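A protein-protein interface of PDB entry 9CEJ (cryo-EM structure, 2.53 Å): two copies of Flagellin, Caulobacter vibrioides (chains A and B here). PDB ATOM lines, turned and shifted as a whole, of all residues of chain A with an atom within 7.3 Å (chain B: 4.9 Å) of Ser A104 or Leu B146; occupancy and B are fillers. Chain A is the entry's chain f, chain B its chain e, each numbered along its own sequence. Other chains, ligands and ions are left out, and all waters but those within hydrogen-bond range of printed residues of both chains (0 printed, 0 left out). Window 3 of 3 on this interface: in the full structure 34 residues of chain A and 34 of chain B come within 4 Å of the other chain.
The backbone carbonyl oxygen (O) of Asn B134 sits close to the side-chain amide oxygen (OD1) of Asn A106 (2.7 Å).
OD1 of Asp A102 sits close to O of Thr B147 (2.8 Å).
OG of Ser A104 sits at hydrogen-bond distance from NH2 of Arg B71 (3.0 Å).
NH2 of Arg B71 lies within salt-bridge range of OD2 of Asp A102.
The backbone carbonyl oxygen of Phe B148 is in hydrogen-bond range of the backbone NH of Phe B157 (2.6 Å).
The side-chain carboxylate of Asp A102 is in hydrogen-bond range of the side-chain hydroxyl of Ser A104.
The backbone NH (N) of Val B159 sits at hydrogen-bond distance from the backbone carbonyl oxygen (O) of Leu B146 (3.1 Å).
OG of Ser A109 lies within hydrogen-bond range of O of Asn A106, at 3.2 Å.
Among the printed residues, pairs that only touch across the chains: Asp A102 with Phe B148 (3.7 Å), Thr A103 with Thr B147 (3.6 Å), Ser A104 with Val B136 (3.2 Å), Ser A104 with Leu B146 (3.8 Å), Ser A104 with Phe B148 (3.3 Å), Leu A105 with Arg B71 (3.5 Å) and Asn A106 with Val B136 (3.5 Å).
Of the printed residues of chain B, Asp A102 touches Arg B71 (2.6 Å), Thr B147 (2.8 Å) and Phe B148 (3.7 Å).
Of the printed residues of chain B, Ser A104 touches Arg B71 (3.0 Å), Val B136 (3.2 Å), Leu B146 (3.8 Å) and Phe B148 (3.3 Å).
Printed residues of chain B within 4 Å of Leu A105: Arg B71 (3.5 Å).
Of the printed residues of chain A, Val B136 touches Ser A104 (3.2 Å) and Asn A106 (3.5 Å).
Lys B145 touches none of the printed residues of chain A.
Leu B146 touches one residue of chain A.
Printed residues of chain A within 4 Å of Thr B147: Asp A102 (2.8 Å) and Thr A103 (3.6 Å).
Of the printed residues of chain A, Phe B148 touches Asp A102 (3.7 Å) and Ser A104 (3.3 Å).
The nearest residue of chain A that does not touch Leu B146 is Thr A103 (4.2 Å).
The nearest printed residue of chain A that does not touch Asn B134 is Ser A104 (4.5 Å).
Of the 14 printed residues of chain B, 6 touch a printed residue of chain A.
No position is printed for both chains.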
ATOM      1  N   ALA A  99      22.491   6.072 -15.550  1.00  0.00           N
ATOM      2  CA  ALA A  99      21.075   5.903 -15.249  1.00  0.00           C
ATOM      3  C   ALA A  99      20.837   4.686 -14.366  1.00  0.00           C
ATOM      4  O   ALA A  99      19.950   4.702 -13.507  1.00  0.00           O
ATOM      5  CB  ALA A  99      20.273   5.791 -16.543  1.00  0.00           C
ATOM      6  N   SER A 101      22.821   3.509 -12.101  1.00  0.00           N
ATOM      7  CA  SER A 101      23.262   3.744 -10.733  1.00  0.00           C
ATOM      8  C   SER A 101      22.124   4.159  -9.808  1.00  0.00           C
ATOM      9  O   SER A 101      22.226   3.946  -8.596  1.00  0.00           O
ATOM     10  CB  SER A 101      24.356   4.812 -10.700  1.00  0.00           C
ATOM     11  OG  SER A 101      24.765   5.068  -9.370  1.00  0.00           O
ATOM     12  N   ASP A 102      21.053   4.742 -10.345  1.00  0.00           N
ATOM     13  CA  ASP A 102      19.947   5.195  -9.513  1.00  0.00           C
ATOM     14  C   ASP A 102      19.258   4.013  -8.837  1.00  0.00           C
ATOM     15  O   ASP A 102      19.004   2.977  -9.458  1.00  0.00           O
ATOM     16  CB  ASP A 102      18.950   5.983 -10.364  1.00  0.00           C
ATOM     17  CG  ASP A 102      17.870   6.655  -9.538  1.00  0.00           C
ATOM     18  OD1 ASP A 102      17.859   6.493  -8.301  1.00  0.00           O
ATOM     19  OD2 ASP A 102      17.022   7.349 -10.135  1.00  0.00           O
ATOM     20  N   THR A 103      18.951   4.180  -7.553  1.00  0.00           N
ATOM     21  CA  THR A 103      18.307   3.148  -6.754  1.00  0.00           C
ATOM     22  C   THR A 103      16.786   3.164  -6.846  1.00  0.00           C
ATOM     23  O   THR A 103      16.146   2.196  -6.424  1.00  0.00           O
ATOM     24  CB  THR A 103      18.731   3.285  -5.287  1.00  0.00           C
ATOM     25  OG1 THR A 103      18.176   4.487  -4.736  1.00  0.00           O
ATOM     26  CG2 THR A 103      20.244   3.342  -5.179  1.00  0.00           C
ATOM     27  N   SER A 104      16.189   4.232  -7.376  1.00  0.00           N
ATOM     28  CA  SER A 104      14.735   4.326  -7.457  1.00  0.00           C
ATOM     29  C   SER A 104      14.127   3.447  -8.544  1.00  0.00           C
ATOM     30  O   SER A 104      12.928   3.153  -8.478  1.00  0.00           O
ATOM     31  CB  SER A 104      14.309   5.781  -7.680  1.00  0.00           C
ATOM     32  OG  SER A 104      14.992   6.354  -8.777  1.00  0.00           O
ATOM     33  N   LEU A 105      14.901   3.047  -9.546  1.00  0.00           N
ATOM     34  CA  LEU A 105      14.412   2.160 -10.590  1.00  0.00           C
ATOM     35  C   LEU A 105      14.370   0.711 -10.111  1.00  0.00           C
ATOM     36  O   LEU A 105      15.148   0.295  -9.248  1.00  0.00           O
ATOM     37  CB  LEU A 105      15.268   2.304 -11.852  1.00  0.00           C
ATOM     38  CG  LEU A 105      16.766   1.985 -11.839  1.00  0.00           C
ATOM     39  CD1 LEU A 105      17.039   0.510 -12.011  1.00  0.00           C
ATOM     40  CD2 LEU A 105      17.467   2.782 -12.924  1.00  0.00           C
ATOM     41  N   ASN A 106      13.439  -0.054 -10.682  1.00  0.00           N
ATOM     42  CA  ASN A 106      13.240  -1.455 -10.342  1.00  0.00           C
ATOM     43  C   ASN A 106      14.063  -2.370 -11.247  1.00  0.00           C
ATOM     44  O   ASN A 106      14.720  -1.935 -12.196  1.00  0.00           O
ATOM     45  CB  ASN A 106      11.756  -1.806 -10.388  1.00  0.00           C
ATOM     46  CG  ASN A 106      11.009  -1.298  -9.177  1.00  0.00           C
ATOM     47  OD1 ASN A 106      11.038  -0.109  -8.871  1.00  0.00           O
ATOM     48  ND2 ASN A 106      10.339  -2.203  -8.473  1.00  0.00           N
ATOM     49  N   SER A 109      14.172  -2.409 -15.523  1.00  0.00           N
ATOM     50  CA  SER A 109      14.981  -1.421 -16.228  1.00  0.00           C
ATOM     51  C   SER A 109      16.465  -1.609 -15.949  1.00  0.00           C
ATOM     52  O   SER A 109      17.297  -1.371 -16.830  1.00  0.00           O
ATOM     53  CB  SER A 109      14.536  -0.009 -15.840  1.00  0.00           C
ATOM     54  OG  SER A 109      14.804   0.252 -14.474  1.00  0.00           O
ATOM     55  N   ALA A 180      23.575  -1.458  -8.142  1.00  0.00           N
ATOM     56  CA  ALA A 180      23.679  -0.031  -8.434  1.00  0.00           C
ATOM     57  C   ALA A 180      25.008   0.545  -7.960  1.00  0.00           C
ATOM     58  O   ALA A 180      25.559   1.455  -8.597  1.00  0.00           O
ATOM     59  CB  ALA A 180      22.512   0.719  -7.794  1.00  0.00           C
ATOM     60  N   ARG B  71      11.664  11.193 -12.385  1.00  0.00           N
ATOM     61  CA  ARG B  71      11.087  10.146 -11.544  1.00  0.00           C
ATOM     62  C   ARG B  71      10.963  10.604 -10.097  1.00  0.00           C
ATOM     63  O   ARG B  71       9.992  10.260  -9.406  1.00  0.00           O
ATOM     64  CB  ARG B  71      11.925   8.870 -11.626  1.00  0.00           C
ATOM     65  CG  ARG B  71      12.413   8.529 -13.017  1.00  0.00           C
ATOM     66  CD  ARG B  71      12.592   7.035 -13.194  1.00  0.00           C
ATOM     67  NE  ARG B  71      13.589   6.511 -12.269  1.00  0.00           N
ATOM     68  CZ  ARG B  71      14.849   6.259 -12.593  1.00  0.00           C
ATOM     69  NH1 ARG B  71      15.305   6.477 -13.816  1.00  0.00           N
ATOM     70  NH2 ARG B  71      15.674   5.783 -11.665  1.00  0.00           N
ATOM     71  N   ASN B 134       6.101   3.394  -9.835  1.00  0.00           N
ATOM     72  CA  ASN B 134       7.043   2.507 -10.518  1.00  0.00           C
ATOM     73  C   ASN B 134       7.750   1.595  -9.515  1.00  0.00           C
ATOM     74  O   ASN B 134       8.965   1.405  -9.559  1.00  0.00           O
ATOM     75  CB  ASN B 134       8.049   3.316 -11.344  1.00  0.00           C
ATOM     76  CG  ASN B 134       8.919   2.448 -12.248  1.00  0.00           C
ATOM     77  OD1 ASN B 134       8.808   1.222 -12.258  1.00  0.00           O
ATOM     78  ND2 ASN B 134       9.802   3.091 -13.003  1.00  0.00           N
ATOM     79  N   VAL B 136       8.344   1.894  -6.273  1.00  0.00           N
ATOM     80  CA  VAL B 136       9.047   2.478  -5.138  1.00  0.00           C
ATOM     81  C   VAL B 136       8.202   3.604  -4.567  1.00  0.00           C
ATOM     82  O   VAL B 136       7.345   4.173  -5.249  1.00  0.00           O
ATOM     83  CB  VAL B 136      10.452   3.001  -5.516  1.00  0.00           C
ATOM     84  CG1 VAL B 136      11.334   1.865  -6.004  1.00  0.00           C
ATOM     85  CG2 VAL B 136      10.352   4.100  -6.561  1.00  0.00           C
ATOM     86  N   SER B 137       8.445   3.922  -3.300  1.00  0.00           N
ATOM     87  CA  SER B 137       7.694   4.955  -2.605  1.00  0.00           C
ATOM     88  C   SER B 137       8.576   5.641  -1.574  1.00  0.00           C
ATOM     89  O   SER B 137       9.329   4.985  -0.849  1.00  0.00           O
ATOM     90  CB  SER B 137       6.463   4.368  -1.918  1.00  0.00           C
ATOM     91  OG  SER B 137       5.927   5.275  -0.973  1.00  0.00           O
ATOM     92  N   ILE B 138       8.475   6.970  -1.520  1.00  0.00           N
ATOM     93  CA  ILE B 138       9.172   7.759  -0.512  1.00  0.00           C
ATOM     94  C   ILE B 138       8.375   7.869   0.783  1.00  0.00           C
ATOM     95  O   ILE B 138       8.933   8.288   1.809  1.00  0.00           O
ATOM     96  CB  ILE B 138       9.506   9.165  -1.063  1.00  0.00           C
ATOM     97  CG1 ILE B 138      10.506   9.902  -0.170  1.00  0.00           C
ATOM     98  CG2 ILE B 138       8.241   9.991  -1.212  1.00  0.00           C
ATOM     99  CD1 ILE B 138      11.875   9.263  -0.133  1.00  0.00           C
ATOM    100  N   THR B 143      11.715   2.241   2.757  1.00  0.00           N
ATOM    101  CA  THR B 143      13.132   2.540   2.622  1.00  0.00           C
ATOM    102  C   THR B 143      13.445   3.812   3.394  1.00  0.00           C
ATOM    103  O   THR B 143      12.571   4.649   3.632  1.00  0.00           O
ATOM    104  CB  THR B 143      13.542   2.686   1.150  1.00  0.00           C
ATOM    105  OG1 THR B 143      14.968   2.809   1.057  1.00  0.00           O
ATOM    106  CG2 THR B 143      12.891   3.911   0.530  1.00  0.00           C
ATOM    107  N   THR B 144      14.708   3.937   3.807  1.00  0.00           N
ATOM    108  CA  THR B 144      15.127   5.103   4.577  1.00  0.00           C
ATOM    109  C   THR B 144      15.361   6.320   3.691  1.00  0.00           C
ATOM    110  O   THR B 144      15.113   7.455   4.114  1.00  0.00           O
ATOM    111  CB  THR B 144      16.393   4.783   5.372  1.00  0.00           C
ATOM    112  OG1 THR B 144      17.418   4.333   4.476  1.00  0.00           O
ATOM    113  CG2 THR B 144      16.119   3.705   6.403  1.00  0.00           C
ATOM    114  N   LYS B 145      15.831   6.109   2.463  1.00  0.00           N
ATOM    115  CA  LYS B 145      16.157   7.220   1.581  1.00  0.00           C
ATOM    116  C   LYS B 145      16.178   6.734   0.142  1.00  0.00           C
ATOM    117  O   LYS B 145      16.337   5.540  -0.124  1.00  0.00           O
ATOM    118  CB  LYS B 145      17.509   7.846   1.944  1.00  0.00           C
ATOM    119  CG  LYS B 145      18.708   6.975   1.599  1.00  0.00           C
ATOM    120  CD  LYS B 145      19.745   6.986   2.705  1.00  0.00           C
ATOM    121  CE  LYS B 145      20.293   8.383   2.923  1.00  0.00           C
ATOM    122  NZ  LYS B 145      21.364   8.412   3.956  1.00  0.00           N
ATOM    123  N   LEU B 146      16.017   7.677  -0.782  1.00  0.00           N
ATOM    124  CA  LEU B 146      16.142   7.421  -2.209  1.00  0.00           C
ATOM    125  C   LEU B 146      17.135   8.416  -2.789  1.00  0.00           C
ATOM    126  O   LEU B 146      17.042   9.617  -2.520  1.00  0.00           O
ATOM    127  CB  LEU B 146      14.788   7.531  -2.913  1.00  0.00           C
ATOM    128  CG  LEU B 146      13.868   6.318  -2.756  1.00  0.00           C
ATOM    129  CD1 LEU B 146      12.406   6.733  -2.754  1.00  0.00           C
ATOM    130  CD2 LEU B 146      14.135   5.286  -3.837  1.00  0.00           C
ATOM    131  N   THR B 147      18.086   7.916  -3.574  1.00  0.00           N
ATOM    132  CA  THR B 147      19.187   8.719  -4.085  1.00  0.00           C
ATOM    133  C   THR B 147      19.059   8.879  -5.593  1.00  0.00           C
ATOM    134  O   THR B 147      19.210   7.909  -6.341  1.00  0.00           O
ATOM    135  CB  THR B 147      20.535   8.087  -3.736  1.00  0.00           C
ATOM    136  OG1 THR B 147      20.769   8.210  -2.327  1.00  0.00           O
ATOM    137  CG2 THR B 147      21.655   8.779  -4.486  1.00  0.00           C
ATOM    138  N   PHE B 148      18.794  10.105  -6.029  1.00  0.00           N
ATOM    139  CA  PHE B 148      18.597  10.445  -7.428  1.00  0.00           C
ATOM    140  C   PHE B 148      19.890  11.006  -8.017  1.00  0.00           C
ATOM    141  O   PHE B 148      20.759  11.516  -7.305  1.00  0.00           O
ATOM    142  CB  PHE B 148      17.441  11.438  -7.560  1.00  0.00           C
ATOM    143  CG  PHE B 148      16.115  10.881  -7.114  1.00  0.00           C
ATOM    144  CD1 PHE B 148      15.603   9.729  -7.682  1.00  0.00           C
ATOM    145  CD2 PHE B 148      15.402  11.495  -6.098  1.00  0.00           C
ATOM    146  CE1 PHE B 148      14.390   9.215  -7.263  1.00  0.00           C
ATOM    147  CE2 PHE B 148      14.192  10.982  -5.673  1.00  0.00           C
ATOM    148  CZ  PHE B 148      13.687   9.841  -6.255  1.00  0.00           C
ATOM    149  N   PHE B 157      21.550  12.777  -5.158  1.00  0.00           N
ATOM    150  CA  PHE B 157      20.703  13.855  -4.645  1.00  0.00           C
ATOM    151  C   PHE B 157      19.774  13.169  -3.643  1.00  0.00           C
ATOM    152  O   PHE B 157      18.661  12.756  -3.971  1.00  0.00           O
ATOM    153  CB  PHE B 157      19.933  14.567  -5.761  1.00  0.00           C
ATOM    154  CG  PHE B 157      19.230  15.831  -5.322  1.00  0.00           C
ATOM    155  CD1 PHE B 157      19.587  17.054  -5.869  1.00  0.00           C
ATOM    156  CD2 PHE B 157      18.218  15.804  -4.377  1.00  0.00           C
ATOM    157  CE1 PHE B 157      18.953  18.219  -5.481  1.00  0.00           C
ATOM    158  CE2 PHE B 157      17.581  16.967  -3.982  1.00  0.00           C
ATOM    159  CZ  PHE B 157      17.949  18.175  -4.536  1.00  0.00           C
ATOM    160  N   THR B 158      20.258  13.020  -2.414  1.00  0.00           N
ATOM    161  CA  THR B 158      19.514  12.289  -1.399  1.00  0.00           C
ATOM    162  C   THR B 158      18.233  13.025  -1.024  1.00  0.00           C
ATOM    163  O   THR B 158      18.217  14.252  -0.902  1.00  0.00           O
ATOM    164  CB  THR B 158      20.389  12.082  -0.160  1.00  0.00           C
ATOM    165  OG1 THR B 158      21.556  11.333  -0.519  1.00  0.00           O
ATOM    166  CG2 THR B 158      19.631  11.328   0.917  1.00  0.00           C
ATOM    167  N   VAL B 159      17.156  12.263  -0.846  1.00  0.00           N
ATOM    168  CA  VAL B 159      15.909  12.760  -0.277  1.00  0.00           C
ATOM    169  C   VAL B 159      15.475  11.775   0.805  1.00  0.00           C
ATOM    170  O   VAL B 159      15.234  10.594   0.525  1.00  0.00           O
ATOM    171  CB  VAL B 159      14.818  12.977  -1.342  1.00  0.00           C
ATOM    172  CG1 VAL B 159      14.386  11.679  -2.014  1.00  0.00           C
ATOM    173  CG2 VAL B 159      13.615  13.686  -0.731  1.00  0.00           C
